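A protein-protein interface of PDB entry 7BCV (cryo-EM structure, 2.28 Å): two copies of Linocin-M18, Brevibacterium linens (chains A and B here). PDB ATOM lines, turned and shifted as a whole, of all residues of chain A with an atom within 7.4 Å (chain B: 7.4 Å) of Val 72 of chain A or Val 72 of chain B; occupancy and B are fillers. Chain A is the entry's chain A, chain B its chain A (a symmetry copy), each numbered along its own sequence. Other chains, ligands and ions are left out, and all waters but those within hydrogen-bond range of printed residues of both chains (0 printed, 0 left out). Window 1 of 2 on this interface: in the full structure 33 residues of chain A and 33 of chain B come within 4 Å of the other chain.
The backbone carbonyl oxygen of Thr 47 of chain A lies within hydrogen-bond range of the guanidinium group of Arg 70 of chain B (3.2 Å).
The side-chain hydroxyl (OG) of Ser 48 of chain A lies within hydrogen-bond range of the side-chain hydroxyl (OG1) of Thr 51 of chain B, at 3.0 Å.
OG of Ser 48 of chain A sits at hydrogen-bond distance from NH1 of Arg 70 of chain B, 3.0 Å away.
The side-chain hydroxyl of Ser 48 of chain B lies within hydrogen-bond range of the side-chain hydroxyl of Thr 51 of chain A.
NE2 of Gln 69 of chain A sits at hydrogen-bond distance from O of Glu 74 of chain B.
O of Ala 126 of chain B is in hydrogen-bond range of NE2 of Gln 69 of chain A (3.1 Å).
The backbone carbonyl oxygen of Thr 47 of chain B lies within hydrogen-bond range of the guanidinium group of Arg 70 of chain A.
The side-chain hydroxyl of Ser 48 of chain B lies within hydrogen-bond range of the guanidinium group of Arg 70 of chain A, 3.0 Å away.
The backbone NH of Arg 70 of chain A sits at hydrogen-bond distance from the backbone carbonyl oxygen of Tyr 75 of chain B (3.0 Å).
The side-chain carboxylate of Glu 74 of chain B lies within hydrogen-bond range of the backbone NH of Val 72 of chain A (3.0 Å).
The backbone carbonyl oxygen (O) of Glu 74 of chain A lies within hydrogen-bond range of the side-chain amide nitrogen (NE2) of Gln 69 of chain B.
The side-chain carboxylate (OE2) of Glu 74 of chain A lies within hydrogen-bond range of the backbone NH (N) of Val 72 of chain B (3.0 Å).
The backbone carbonyl oxygen (O) of Tyr 75 of chain A is in hydrogen-bond range of the backbone NH (N) of Arg 70 of chain B, 3.0 Å away.
The backbone carbonyl oxygen (O) of Ala 126 of chain A lies within hydrogen-bond range of the side-chain amide nitrogen (NE2) of Gln 69 of chain B (3.1 Å).
The side-chain carboxylate (OE2) of Glu 74 of chain B lies close to the backbone carbonyl oxygen (O) of Arg 70 of chain A (3.4 Å).
OE2 of Glu 74 of chain A sits close to O of Arg 70 of chain B (3.4 Å).
The backbone NH (N) of Ile 71 of chain A lies within hydrogen-bond range of the backbone carbonyl oxygen (O) of His 54 of chain A.
O of Ile 71 of chain B lies within hydrogen-bond range of OG1 of Thr 52 of chain B.
Among the printed residues, merely in contact across the chains: Ser 48 of chain A with Val 72 of chain B, Ala 49 of chain A with Val 72 of chain B, Gln 69 of chain A with Tyr 75 of chain B, Ile 71 of chain A with Glu 74 of chain B, Val 72 of chain A with Ser 48 of chain B, Val 72 of chain A with Ala 49 of chain B, Val 72 of chain A with Val 72 of chain B, Glu 74 of chain A with Ile 71 of chain B and Tyr 75 of chain A with Gln 69 of chain B.
Of chain B, only Ser 48, Ala 49, Val 72 and Glu 74 come within 4 Å of Val 72 of chain A.
Of the printed residues of chain A, Val 72 of chain B touches Ser 48, Ala 49, Val 72 and Glu 74.
Of the printed residues of chain A, Thr 47 of chain B touches Arg 70 (3.2 Å).
Of the printed residues of chain A, Tyr 75 of chain B touches Gln 69 (3.5 Å) and Arg 70 (3.0 Å).
His 54 of chain A touches none of the printed residues of chain B.
The nearest residue of chain B that does not touch Val 72 of chain A is Gln 73 of chain B (6.3 Å).
The nearest residue of chain A that does not touch Val 72 of chain B is Gln 73 of chain A (6.3 Å).
Of the 19 printed residues of chain A, 11 touch a printed residue of chain B.
Printed residues of chain A that touch a printed residue of chain B: Thr 47, Ser 48, Ala 49, Thr 51, Gln 69, Arg 70, Ile 71, Val 72, Glu 74, Tyr 75 and Ala 126.
Hydrophobic or aromatic side chains of chain A that line the printed part of chain B: Ala 49, Val 72 and Ala 126.
Hydrophobic or aromatic side chains of chain B within 4 Å of the printed part of chain A: Ala 49, Val 72 and Ala 126.
Along chain B the printed residues that touch a printed residue of chain A span positions 47 to 126.
Among the printed residues, no Asp or Glu carboxylate lies within 4 Å of a Lys or Arg side-chain nitrogen of the other chain.
Thr 47 of chain A touches Arg 70 of chain B, and with the chains exchanged Arg 70 of chain A touches Thr 47 of chain B.
Gln 69 of chain A touches Tyr 75 of chain B, and with the chains exchanged Tyr 75 of chain A touches Gln 69 of chain B.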
ATOM      1  N   THR A  47      26.837   0.482 -19.709  1.00  0.00           N
ATOM      2  CA  THR A  47      25.802   1.501 -19.597  1.00  0.00           C
ATOM      3  C   THR A  47      24.531   0.931 -18.982  1.00  0.00           C
ATOM      4  O   THR A  47      24.140  -0.211 -19.228  1.00  0.00           O
ATOM      5  CB  THR A  47      25.508   2.154 -20.953  1.00  0.00           C
ATOM      6  OG1 THR A  47      24.393   3.044 -20.829  1.00  0.00           O
ATOM      7  CG2 THR A  47      25.192   1.144 -21.980  1.00  0.00           C
ATOM      8  N   SER A  48      23.891   1.742 -18.165  1.00  0.00           N
ATOM      9  CA  SER A  48      22.876   1.257 -17.252  1.00  0.00           C
ATOM     10  C   SER A  48      21.573   2.016 -17.295  1.00  0.00           C
ATOM     11  O   SER A  48      20.576   1.500 -16.788  1.00  0.00           O
ATOM     12  CB  SER A  48      23.407   1.286 -15.819  1.00  0.00           C
ATOM     13  OG  SER A  48      24.474   0.391 -15.668  1.00  0.00           O
ATOM     14  N   ALA A  49      21.533   3.207 -17.876  1.00  0.00           N
ATOM     15  CA  ALA A  49      20.333   4.015 -17.829  1.00  0.00           C
ATOM     16  C   ALA A  49      20.350   4.995 -18.985  1.00  0.00           C
ATOM     17  O   ALA A  49      21.401   5.328 -19.528  1.00  0.00           O
ATOM     18  CB  ALA A  49      20.200   4.764 -16.496  1.00  0.00           C
ATOM     19  N   VAL A  50      19.161   5.430 -19.364  1.00  0.00           N
ATOM     20  CA  VAL A  50      18.960   6.572 -20.240  1.00  0.00           C
ATOM     21  C   VAL A  50      18.004   7.512 -19.519  1.00  0.00           C
ATOM     22  O   VAL A  50      17.017   7.065 -18.928  1.00  0.00           O
ATOM     23  CB  VAL A  50      18.450   6.149 -21.640  1.00  0.00           C
ATOM     24  CG1 VAL A  50      17.193   5.291 -21.564  1.00  0.00           C
ATOM     25  CG2 VAL A  50      18.227   7.357 -22.538  1.00  0.00           C
ATOM     26  N   THR A  51      18.356   8.796 -19.477  1.00  0.00           N
ATOM     27  CA  THR A  51      17.526   9.775 -18.793  1.00  0.00           C
ATOM     28  C   THR A  51      16.245  10.051 -19.573  1.00  0.00           C
ATOM     29  O   THR A  51      16.191   9.935 -20.798  1.00  0.00           O
ATOM     30  CB  THR A  51      18.292  11.089 -18.556  1.00  0.00           C
ATOM     31  OG1 THR A  51      17.477  11.975 -17.789  1.00  0.00           O
ATOM     32  CG2 THR A  51      18.662  11.784 -19.851  1.00  0.00           C
ATOM     33  N   THR A  52      15.195  10.382 -18.843  1.00  0.00           N
ATOM     34  CA  THR A  52      14.005  10.916 -19.477  1.00  0.00           C
ATOM     35  C   THR A  52      14.023  12.434 -19.545  1.00  0.00           C
ATOM     36  O   THR A  52      13.130  13.028 -20.157  1.00  0.00           O
ATOM     37  CB  THR A  52      12.749  10.438 -18.741  1.00  0.00           C
ATOM     38  OG1 THR A  52      12.689  11.039 -17.446  1.00  0.00           O
ATOM     39  CG2 THR A  52      12.769   8.935 -18.599  1.00  0.00           C
ATOM     40  N   GLY A  53      15.035  13.066 -18.955  1.00  0.00           N
ATOM     41  CA  GLY A  53      15.123  14.504 -18.847  1.00  0.00           C
ATOM     42  C   GLY A  53      14.085  15.153 -17.969  1.00  0.00           C
ATOM     43  O   GLY A  53      13.889  16.359 -18.066  1.00  0.00           O
ATOM     44  N   HIS A  54      13.385  14.390 -17.146  1.00  0.00           N
ATOM     45  CA  HIS A  54      12.395  14.922 -16.228  1.00  0.00           C
ATOM     46  C   HIS A  54      12.899  14.811 -14.798  1.00  0.00           C
ATOM     47  O   HIS A  54      13.733  13.966 -14.476  1.00  0.00           O
ATOM     48  CB  HIS A  54      11.062  14.190 -16.379  1.00  0.00           C
ATOM     49  CG  HIS A  54      10.483  14.282 -17.752  1.00  0.00           C
ATOM     50  ND1 HIS A  54       9.799  13.243 -18.339  1.00  0.00           N
ATOM     51  CD2 HIS A  54      10.496  15.285 -18.660  1.00  0.00           C
ATOM     52  CE1 HIS A  54       9.409  13.603 -19.546  1.00  0.00           C
ATOM     53  NE2 HIS A  54       9.824  14.837 -19.767  1.00  0.00           N
ATOM     54  N   ARG A  56      11.759  15.285 -10.393  1.00  0.00           N
ATOM     55  CA  ARG A  56      10.735  14.890  -9.447  1.00  0.00           C
ATOM     56  C   ARG A  56      11.042  15.557  -8.115  1.00  0.00           C
ATOM     57  O   ARG A  56      12.205  15.637  -7.720  1.00  0.00           O
ATOM     58  CB  ARG A  56      10.707  13.368  -9.300  1.00  0.00           C
ATOM     59  CG  ARG A  56       9.611  12.836  -8.443  1.00  0.00           C
ATOM     60  CD  ARG A  56       9.860  11.382  -8.117  1.00  0.00           C
ATOM     61  NE  ARG A  56      10.797  11.235  -7.014  1.00  0.00           N
ATOM     62  CZ  ARG A  56      12.005  10.699  -7.127  1.00  0.00           C
ATOM     63  NH1 ARG A  56      12.786  10.605  -6.060  1.00  0.00           N
ATOM     64  NH2 ARG A  56      12.430  10.249  -8.301  1.00  0.00           N
ATOM     65  N   GLN A  69      14.980  15.283  -7.936  1.00  0.00           N
ATOM     66  CA  GLN A  69      15.718  14.098  -8.344  1.00  0.00           C
ATOM     67  C   GLN A  69      15.418  13.840  -9.809  1.00  0.00           C
ATOM     68  O   GLN A  69      14.256  13.886 -10.215  1.00  0.00           O
ATOM     69  CB  GLN A  69      15.365  12.863  -7.504  1.00  0.00           C
ATOM     70  CG  GLN A  69      16.253  11.650  -7.821  1.00  0.00           C
ATOM     71  CD  GLN A  69      16.432  10.674  -6.663  1.00  0.00           C
ATOM     72  OE1 GLN A  69      15.483  10.342  -5.966  1.00  0.00           O
ATOM     73  NE2 GLN A  69      17.654  10.199  -6.474  1.00  0.00           N
ATOM     74  N   ARG A  70      16.466  13.586 -10.588  1.00  0.00           N
ATOM     75  CA  ARG A  70      16.330  13.178 -11.979  1.00  0.00           C
ATOM     76  C   ARG A  70      15.580  11.855 -12.089  1.00  0.00           C
ATOM     77  O   ARG A  70      15.494  11.075 -11.144  1.00  0.00           O
ATOM     78  CB  ARG A  70      17.701  13.042 -12.637  1.00  0.00           C
ATOM     79  CG  ARG A  70      18.467  14.342 -12.764  1.00  0.00           C
ATOM     80  CD  ARG A  70      17.842  15.278 -13.768  1.00  0.00           C
ATOM     81  NE  ARG A  70      18.529  16.562 -13.793  1.00  0.00           N
ATOM     82  CZ  ARG A  70      19.529  16.858 -14.610  1.00  0.00           C
ATOM     83  NH1 ARG A  70      19.965  15.966 -15.493  1.00  0.00           N
ATOM     84  NH2 ARG A  70      20.087  18.050 -14.553  1.00  0.00           N
ATOM     85  N   ILE A  71      15.001  11.620 -13.256  1.00  0.00           N
ATOM     86  CA  ILE A  71      14.250  10.401 -13.530  1.00  0.00           C
ATOM     87  C   ILE A  71      14.887   9.730 -14.732  1.00  0.00           C
ATOM     88  O   ILE A  71      14.956  10.325 -15.810  1.00  0.00           O
ATOM     89  CB  ILE A  71      12.763  10.685 -13.789  1.00  0.00           C
ATOM     90  CG1 ILE A  71      12.105  11.300 -12.555  1.00  0.00           C
ATOM     91  CG2 ILE A  71      12.046   9.421 -14.247  1.00  0.00           C
ATOM     92  CD1 ILE A  71      10.678  11.703 -12.774  1.00  0.00           C
ATOM     93  N   VAL A  72      15.354   8.502 -14.556  1.00  0.00           N
ATOM     94  CA  VAL A  72      15.941   7.745 -15.651  1.00  0.00           C
ATOM     95  C   VAL A  72      15.144   6.467 -15.854  1.00  0.00           C
ATOM     96  O   VAL A  72      14.286   6.106 -15.055  1.00  0.00           O
ATOM     97  CB  VAL A  72      17.426   7.411 -15.419  1.00  0.00           C
ATOM     98  CG1 VAL A  72      18.263   8.663 -15.299  1.00  0.00           C
ATOM     99  CG2 VAL A  72      17.569   6.523 -14.203  1.00  0.00           C
ATOM    100  N   GLN A  73      15.442   5.784 -16.949  1.00  0.00           N
ATOM    101  CA  GLN A  73      14.971   4.430 -17.176  1.00  0.00           C
ATOM    102  C   GLN A  73      16.170   3.499 -17.157  1.00  0.00           C
ATOM    103  O   GLN A  73      17.046   3.605 -18.016  1.00  0.00           O
ATOM    104  CB  GLN A  73      14.224   4.307 -18.498  1.00  0.00           C
ATOM    105  CG  GLN A  73      13.640   2.932 -18.687  1.00  0.00           C
ATOM    106  CD  GLN A  73      13.256   2.665 -20.102  1.00  0.00           C
ATOM    107  OE1 GLN A  73      14.069   2.234 -20.895  1.00  0.00           O
ATOM    108  NE2 GLN A  73      12.002   2.917 -20.432  1.00  0.00           N
ATOM    109  N   GLU A  74      16.203   2.601 -16.178  1.00  0.00           N
ATOM    110  CA  GLU A  74      17.274   1.624 -16.077  1.00  0.00           C
ATOM    111  C   GLU A  74      17.146   0.535 -17.135  1.00  0.00           C
ATOM    112  O   GLU A  74      16.058   0.008 -17.380  1.00  0.00           O
ATOM    113  CB  GLU A  74      17.271   0.990 -14.694  1.00  0.00           C
ATOM    114  CG  GLU A  74      17.777   1.894 -13.611  1.00  0.00           C
ATOM    115  CD  GLU A  74      17.119   1.641 -12.276  1.00  0.00           C
ATOM    116  OE1 GLU A  74      15.952   1.208 -12.262  1.00  0.00           O
ATOM    117  OE2 GLU A  74      17.761   1.891 -11.240  1.00  0.00           O
ATOM    118  N   TYR A  75      18.277   0.199 -17.745  1.00  0.00           N
ATOM    119  CA  TYR A  75      18.327  -0.798 -18.805  1.00  0.00           C
ATOM    120  C   TYR A  75      17.951  -2.174 -18.277  1.00  0.00           C
ATOM    121  O   TYR A  75      18.242  -2.536 -17.138  1.00  0.00           O
ATOM    122  CB  TYR A  75      19.720  -0.879 -19.416  1.00  0.00           C
ATOM    123  CG  TYR A  75      20.102   0.193 -20.406  1.00  0.00           C
ATOM    124  CD1 TYR A  75      19.468   1.437 -20.437  1.00  0.00           C
ATOM    125  CD2 TYR A  75      21.132  -0.033 -21.289  1.00  0.00           C
ATOM    126  CE1 TYR A  75      19.856   2.406 -21.322  1.00  0.00           C
ATOM    127  CE2 TYR A  75      21.513   0.919 -22.186  1.00  0.00           C
ATOM    128  CZ  TYR A  75      20.881   2.133 -22.198  1.00  0.00           C
ATOM    129  OH  TYR A  75      21.296   3.055 -23.110  1.00  0.00           O
ATOM    130  N   ALA A 126       9.361  -3.615 -15.073  1.00  0.00           N
ATOM    131  CA  ALA A 126      10.573  -2.816 -15.148  1.00  0.00           C
ATOM    132  C   ALA A 126      10.310  -1.363 -15.520  1.00  0.00           C
ATOM    133  O   ALA A 126      11.258  -0.585 -15.643  1.00  0.00           O
ATOM    134  CB  ALA A 126      11.547  -3.432 -16.150  1.00  0.00           C
ATOM    135  N   GLY A 127       9.051  -0.974 -15.685  1.00  0.00           N
ATOM    136  CA  GLY A 127       8.738   0.390 -16.036  1.00  0.00           C
ATOM    137  C   GLY A 127       9.056   0.774 -17.459  1.00  0.00           C
ATOM    138  O   GLY A 127       9.308   1.951 -17.720  1.00  0.00           O
ATOM    139  N   LEU A 254      12.565   4.148 -24.906  1.00  0.00           N
ATOM    140  CA  LEU A 254      11.753   5.328 -24.615  1.00  0.00           C
ATOM    141  C   LEU A 254      10.786   5.596 -25.760  1.00  0.00           C
ATOM    142  O   LEU A 254      11.210   5.812 -26.897  1.00  0.00           O
ATOM    143  CB  LEU A 254      12.632   6.559 -24.386  1.00  0.00           C
ATOM    144  CG  LEU A 254      13.538   6.577 -23.163  1.00  0.00           C
ATOM    145  CD1 LEU A 254      14.418   7.805 -23.183  1.00  0.00           C
ATOM    146  CD2 LEU A 254      12.713   6.504 -21.906  1.00  0.00           C
ATOM    147  N   THR B  47      23.792  15.133 -17.215  1.00  0.00           N
ATOM    148  CA  THR B  47      23.949  13.811 -16.623  1.00  0.00           C
ATOM    149  C   THR B  47      22.993  13.614 -15.453  1.00  0.00           C
ATOM    150  O   THR B  47      22.717  14.527 -14.673  1.00  0.00           O
ATOM    151  CB  THR B  47      25.398  13.556 -16.193  1.00  0.00           C
ATOM    152  OG1 THR B  47      25.482  12.310 -15.490  1.00  0.00           O
ATOM    153  CG2 THR B  47      25.895  14.628 -15.312  1.00  0.00           C
ATOM    154  N   SER B  48      22.479  12.406 -15.345  1.00  0.00           N
ATOM    155  CA  SER B  48      21.321  12.143 -14.516  1.00  0.00           C
ATOM    156  C   SER B  48      21.481  10.990 -13.556  1.00  0.00           C
ATOM    157  O   SER B  48      20.682  10.888 -12.623  1.00  0.00           O
ATOM    158  CB  SER B  48      20.100  11.876 -15.396  1.00  0.00           C
ATOM    159  OG  SER B  48      19.757  13.020 -16.127  1.00  0.00           O
ATOM    160  N   ALA B  49      22.470  10.125 -13.736  1.00  0.00           N
ATOM    161  CA  ALA B  49      22.580   8.943 -12.909  1.00  0.00           C
ATOM    162  C   ALA B  49      24.018   8.464 -12.919  1.00  0.00           C
ATOM    163  O   ALA B  49      24.785   8.757 -13.834  1.00  0.00           O
ATOM    164  CB  ALA B  49      21.642   7.825 -13.383  1.00  0.00           C
ATOM    165  N   VAL B  50      24.372   7.741 -11.871  1.00  0.00           N
ATOM    166  CA  VAL B  50      25.589   6.949 -11.810  1.00  0.00           C
ATOM    167  C   VAL B  50      25.170   5.536 -11.429  1.00  0.00           C
ATOM    168  O   VAL B  50      24.324   5.351 -10.549  1.00  0.00           O
ATOM    169  CB  VAL B  50      26.629   7.554 -10.834  1.00  0.00           C
ATOM    170  CG1 VAL B  50      26.054   7.781  -9.442  1.00  0.00           C
ATOM    171  CG2 VAL B  50      27.889   6.703 -10.767  1.00  0.00           C
ATOM    172  N   THR B  51      25.682   4.549 -12.163  1.00  0.00           N
ATOM    173  CA  THR B  51      25.330   3.163 -11.899  1.00  0.00           C
ATOM    174  C   THR B  51      25.974   2.668 -10.609  1.00  0.00           C
ATOM    175  O   THR B  51      27.036   3.130 -10.192  1.00  0.00           O
ATOM    176  CB  THR B  51      25.731   2.251 -13.072  1.00  0.00           C
ATOM    177  OG1 THR B  51      25.269   0.925 -12.816  1.00  0.00           O
ATOM    178  CG2 THR B  51      27.232   2.200 -13.277  1.00  0.00           C
ATOM    179  N   THR B  52      25.297   1.742  -9.954  1.00  0.00           N
ATOM    180  CA  THR B  52      25.921   1.014  -8.867  1.00  0.00           C
ATOM    181  C   THR B  52      26.580  -0.272  -9.341  1.00  0.00           C
ATOM    182  O   THR B  52      27.247  -0.943  -8.548  1.00  0.00           O
ATOM    183  CB  THR B  52      24.895   0.705  -7.772  1.00  0.00           C
ATOM    184  OG1 THR B  52      23.942  -0.244  -8.256  1.00  0.00           O
ATOM    185  CG2 THR B  52      24.180   1.969  -7.357  1.00  0.00           C
ATOM    186  N   GLY B  53      26.426  -0.608 -10.619  1.00  0.00           N
ATOM    187  CA  GLY B  53      26.902  -1.852 -11.180  1.00  0.00           C
ATOM    188  C   GLY B  53      26.216  -3.095 -10.675  1.00  0.00           C
ATOM    189  O   GLY B  53      26.749  -4.185 -10.848  1.00  0.00           O
ATOM    190  N   HIS B  54      25.074  -2.967 -10.021  1.00  0.00           N
ATOM    191  CA  HIS B  54      24.312  -4.102  -9.535  1.00  0.00           C
ATOM    192  C   HIS B  54      23.035  -4.256 -10.345  1.00  0.00           C
ATOM    193  O   HIS B  54      22.524  -3.300 -10.926  1.00  0.00           O
ATOM    194  CB  HIS B  54      23.982  -3.942  -8.050  1.00  0.00           C
ATOM    195  CG  HIS B  54      25.189  -3.817  -7.181  1.00  0.00           C
ATOM    196  ND1 HIS B  54      25.225  -3.002  -6.075  1.00  0.00           N
ATOM    197  CD2 HIS B  54      26.410  -4.396  -7.263  1.00  0.00           C
ATOM    198  CE1 HIS B  54      26.412  -3.088  -5.507  1.00  0.00           C
ATOM    199  NE2 HIS B  54      27.152  -3.924  -6.211  1.00  0.00           N
ATOM    200  N   ARG B  56      19.056  -6.493 -10.646  1.00  0.00           N
ATOM    201  CA  ARG B  56      17.901  -6.849  -9.845  1.00  0.00           C
ATOM    202  C   ARG B  56      16.991  -7.723 -10.694  1.00  0.00           C
ATOM    203  O   ARG B  56      16.820  -7.461 -11.884  1.00  0.00           O
ATOM    204  CB  ARG B  56      17.168  -5.589  -9.382  1.00  0.00           C
ATOM    205  CG  ARG B  56      16.031  -5.825  -8.449  1.00  0.00           C
ATOM    206  CD  ARG B  56      15.200  -4.572  -8.308  1.00  0.00           C
ATOM    207  NE  ARG B  56      14.266  -4.424  -9.413  1.00  0.00           N
ATOM    208  CZ  ARG B  56      14.322  -3.453 -10.315  1.00  0.00           C
ATOM    209  NH1 ARG B  56      13.420  -3.400 -11.284  1.00  0.00           N
ATOM    210  NH2 ARG B  56      15.273  -2.529 -10.243  1.00  0.00           N
ATOM    211  N   GLN B  69      17.255  -6.003 -14.241  1.00  0.00           N
ATOM    212  CA  GLN B  69      17.263  -4.561 -14.431  1.00  0.00           C
ATOM    213  C   GLN B  69      18.454  -3.995 -13.682  1.00  0.00           C
ATOM    214  O   GLN B  69      18.685  -4.362 -12.529  1.00  0.00           O
ATOM    215  CB  GLN B  69      15.967  -3.893 -13.949  1.00  0.00           C
ATOM    216  CG  GLN B  69      15.902  -2.397 -14.292  1.00  0.00           C
ATOM    217  CD  GLN B  69      14.490  -1.845 -14.462  1.00  0.00           C
ATOM    218  OE1 GLN B  69      13.597  -2.148 -13.683  1.00  0.00           O
ATOM    219  NE2 GLN B  69      14.299  -1.016 -15.477  1.00  0.00           N
ATOM    220  N   ARG B  70      19.207  -3.122 -14.345  1.00  0.00           N
ATOM    221  CA  ARG B  70      20.295  -2.386 -13.718  1.00  0.00           C
ATOM    222  C   ARG B  70      19.776  -1.500 -12.591  1.00  0.00           C
ATOM    223  O   ARG B  70      18.599  -1.155 -12.523  1.00  0.00           O
ATOM    224  CB  ARG B  70      21.026  -1.526 -14.745  1.00  0.00           C
ATOM    225  CG  ARG B  70      21.755  -2.311 -15.816  1.00  0.00           C
ATOM    226  CD  ARG B  70      22.950  -3.051 -15.269  1.00  0.00           C
ATOM    227  NE  ARG B  70      23.568  -3.886 -16.290  1.00  0.00           N
ATOM    228  CZ  ARG B  70      24.563  -3.494 -17.073  1.00  0.00           C
ATOM    229  NH1 ARG B  70      25.077  -2.276 -16.951  1.00  0.00           N
ATOM    230  NH2 ARG B  70      25.052  -4.326 -17.970  1.00  0.00           N
ATOM    231  N   ILE B  71      20.668  -1.156 -11.675  1.00  0.00           N
ATOM    232  CA  ILE B  71      20.339  -0.309 -10.535  1.00  0.00           C
ATOM    233  C   ILE B  71      21.257   0.897 -10.580  1.00  0.00           C
ATOM    234  O   ILE B  71      22.481   0.747 -10.538  1.00  0.00           O
ATOM    235  CB  ILE B  71      20.485  -1.056  -9.200  1.00  0.00           C
ATOM    236  CG1 ILE B  71      19.512  -2.232  -9.127  1.00  0.00           C
ATOM    237  CG2 ILE B  71      20.310  -0.099  -8.027  1.00  0.00           C
ATOM    238  CD1 ILE B  71      19.676  -3.070  -7.896  1.00  0.00           C
ATOM    239  N   VAL B  72      20.680   2.087 -10.668  1.00  0.00           N
ATOM    240  CA  VAL B  72      21.461   3.315 -10.669  1.00  0.00           C
ATOM    241  C   VAL B  72      21.038   4.173  -9.487  1.00  0.00           C
ATOM    242  O   VAL B  72      20.053   3.899  -8.809  1.00  0.00           O
ATOM    243  CB  VAL B  72      21.320   4.112 -11.979  1.00  0.00           C
ATOM    244  CG1 VAL B  72      21.814   3.318 -13.165  1.00  0.00           C
ATOM    245  CG2 VAL B  72      19.886   4.555 -12.159  1.00  0.00           C
ATOM    246  N   GLN B  73      21.808   5.223  -9.250  1.00  0.00           N
ATOM    247  CA  GLN B  73      21.422   6.282  -8.335  1.00  0.00           C
ATOM    248  C   GLN B  73      21.202   7.551  -9.139  1.00  0.00           C
ATOM    249  O   GLN B  73      22.145   8.071  -9.739  1.00  0.00           O
ATOM    250  CB  GLN B  73      22.476   6.511  -7.259  1.00  0.00           C
ATOM    251  CG  GLN B  73      22.031   7.532  -6.245  1.00  0.00           C
ATOM    252  CD  GLN B  73      23.163   8.056  -5.429  1.00  0.00           C
ATOM    253  OE1 GLN B  73      23.826   8.995  -5.821  1.00  0.00           O
ATOM    254  NE2 GLN B  73      23.391   7.452  -4.278  1.00  0.00           N
ATOM    255  N   GLU B  74      19.965   8.034  -9.153  1.00  0.00           N
ATOM    256  CA  GLU B  74      19.635   9.267  -9.848  1.00  0.00           C
ATOM    257  C   GLU B  74      20.156  10.491  -9.104  1.00  0.00           C
ATOM    258  O   GLU B  74      20.026  10.598  -7.883  1.00  0.00           O
ATOM    259  CB  GLU B  74      18.128   9.380 -10.021  1.00  0.00           C
ATOM    260  CG  GLU B  74      17.565   8.457 -11.057  1.00  0.00           C
ATOM    261  CD  GLU B  74      16.162   8.000 -10.739  1.00  0.00           C
ATOM    262  OE1 GLU B  74      15.822   7.914  -9.545  1.00  0.00           O
ATOM    263  OE2 GLU B  74      15.403   7.709 -11.682  1.00  0.00           O
ATOM    264  N   TYR B  75      20.733  11.415  -9.864  1.00  0.00           N
ATOM    265  CA  TYR B  75      21.315  12.629  -9.311  1.00  0.00           C
ATOM    266  C   TYR B  75      20.246  13.508  -8.680  1.00  0.00           C
ATOM    267  O   TYR B  75      19.106  13.577  -9.139  1.00  0.00           O
ATOM    268  CB  TYR B  75      22.029  13.436 -10.388  1.00  0.00           C
ATOM    269  CG  TYR B  75      23.401  12.967 -10.805  1.00  0.00           C
ATOM    270  CD1 TYR B  75      23.830  11.652 -10.610  1.00  0.00           C
ATOM    271  CD2 TYR B  75      24.255  13.843 -11.434  1.00  0.00           C
ATOM    272  CE1 TYR B  75      25.066  11.243 -11.027  1.00  0.00           C
ATOM    273  CE2 TYR B  75      25.496  13.449 -11.836  1.00  0.00           C
ATOM    274  CZ  TYR B  75      25.896  12.155 -11.639  1.00  0.00           C
ATOM    275  OH  TYR B  75      27.143  11.805 -12.058  1.00  0.00           O
ATOM    276  N   ALA B 126      15.601  10.391  -1.273  1.00  0.00           N
ATOM    277  CA  ALA B 126      16.146  10.197  -2.607  1.00  0.00           C
ATOM    278  C   ALA B 126      17.017   8.954  -2.722  1.00  0.00           C
ATOM    279  O   ALA B 126      17.562   8.690  -3.797  1.00  0.00           O
ATOM    280  CB  ALA B 126      16.949  11.425  -3.030  1.00  0.00           C
ATOM    281  N   GLY B 127      17.148   8.176  -1.654  1.00  0.00           N
ATOM    282  CA  GLY B 127      17.959   6.983  -1.702  1.00  0.00           C
ATOM    283  C   GLY B 127      19.448   7.222  -1.727  1.00  0.00           C
ATOM    284  O   GLY B 127      20.180   6.383  -2.255  1.00  0.00           O
ATOM    285  N   LEU B 254      28.022   8.009  -3.967  1.00  0.00           N
ATOM    286  CA  LEU B 254      28.109   6.578  -3.677  1.00  0.00           C
ATOM    287  C   LEU B 254      29.124   6.328  -2.571  1.00  0.00           C
ATOM    288  O   LEU B 254      30.302   6.663  -2.718  1.00  0.00           O
ATOM    289  CB  LEU B 254      28.500   5.786  -4.925  1.00  0.00           C
ATOM    290  CG  LEU B 254      27.517   5.741  -6.086  1.00  0.00           C
ATOM    291  CD1 LEU B 254      28.135   5.028  -7.267  1.00  0.00           C
ATOM    292  CD2 LEU B 254      26.232   5.087  -5.652  1.00  0.00           C
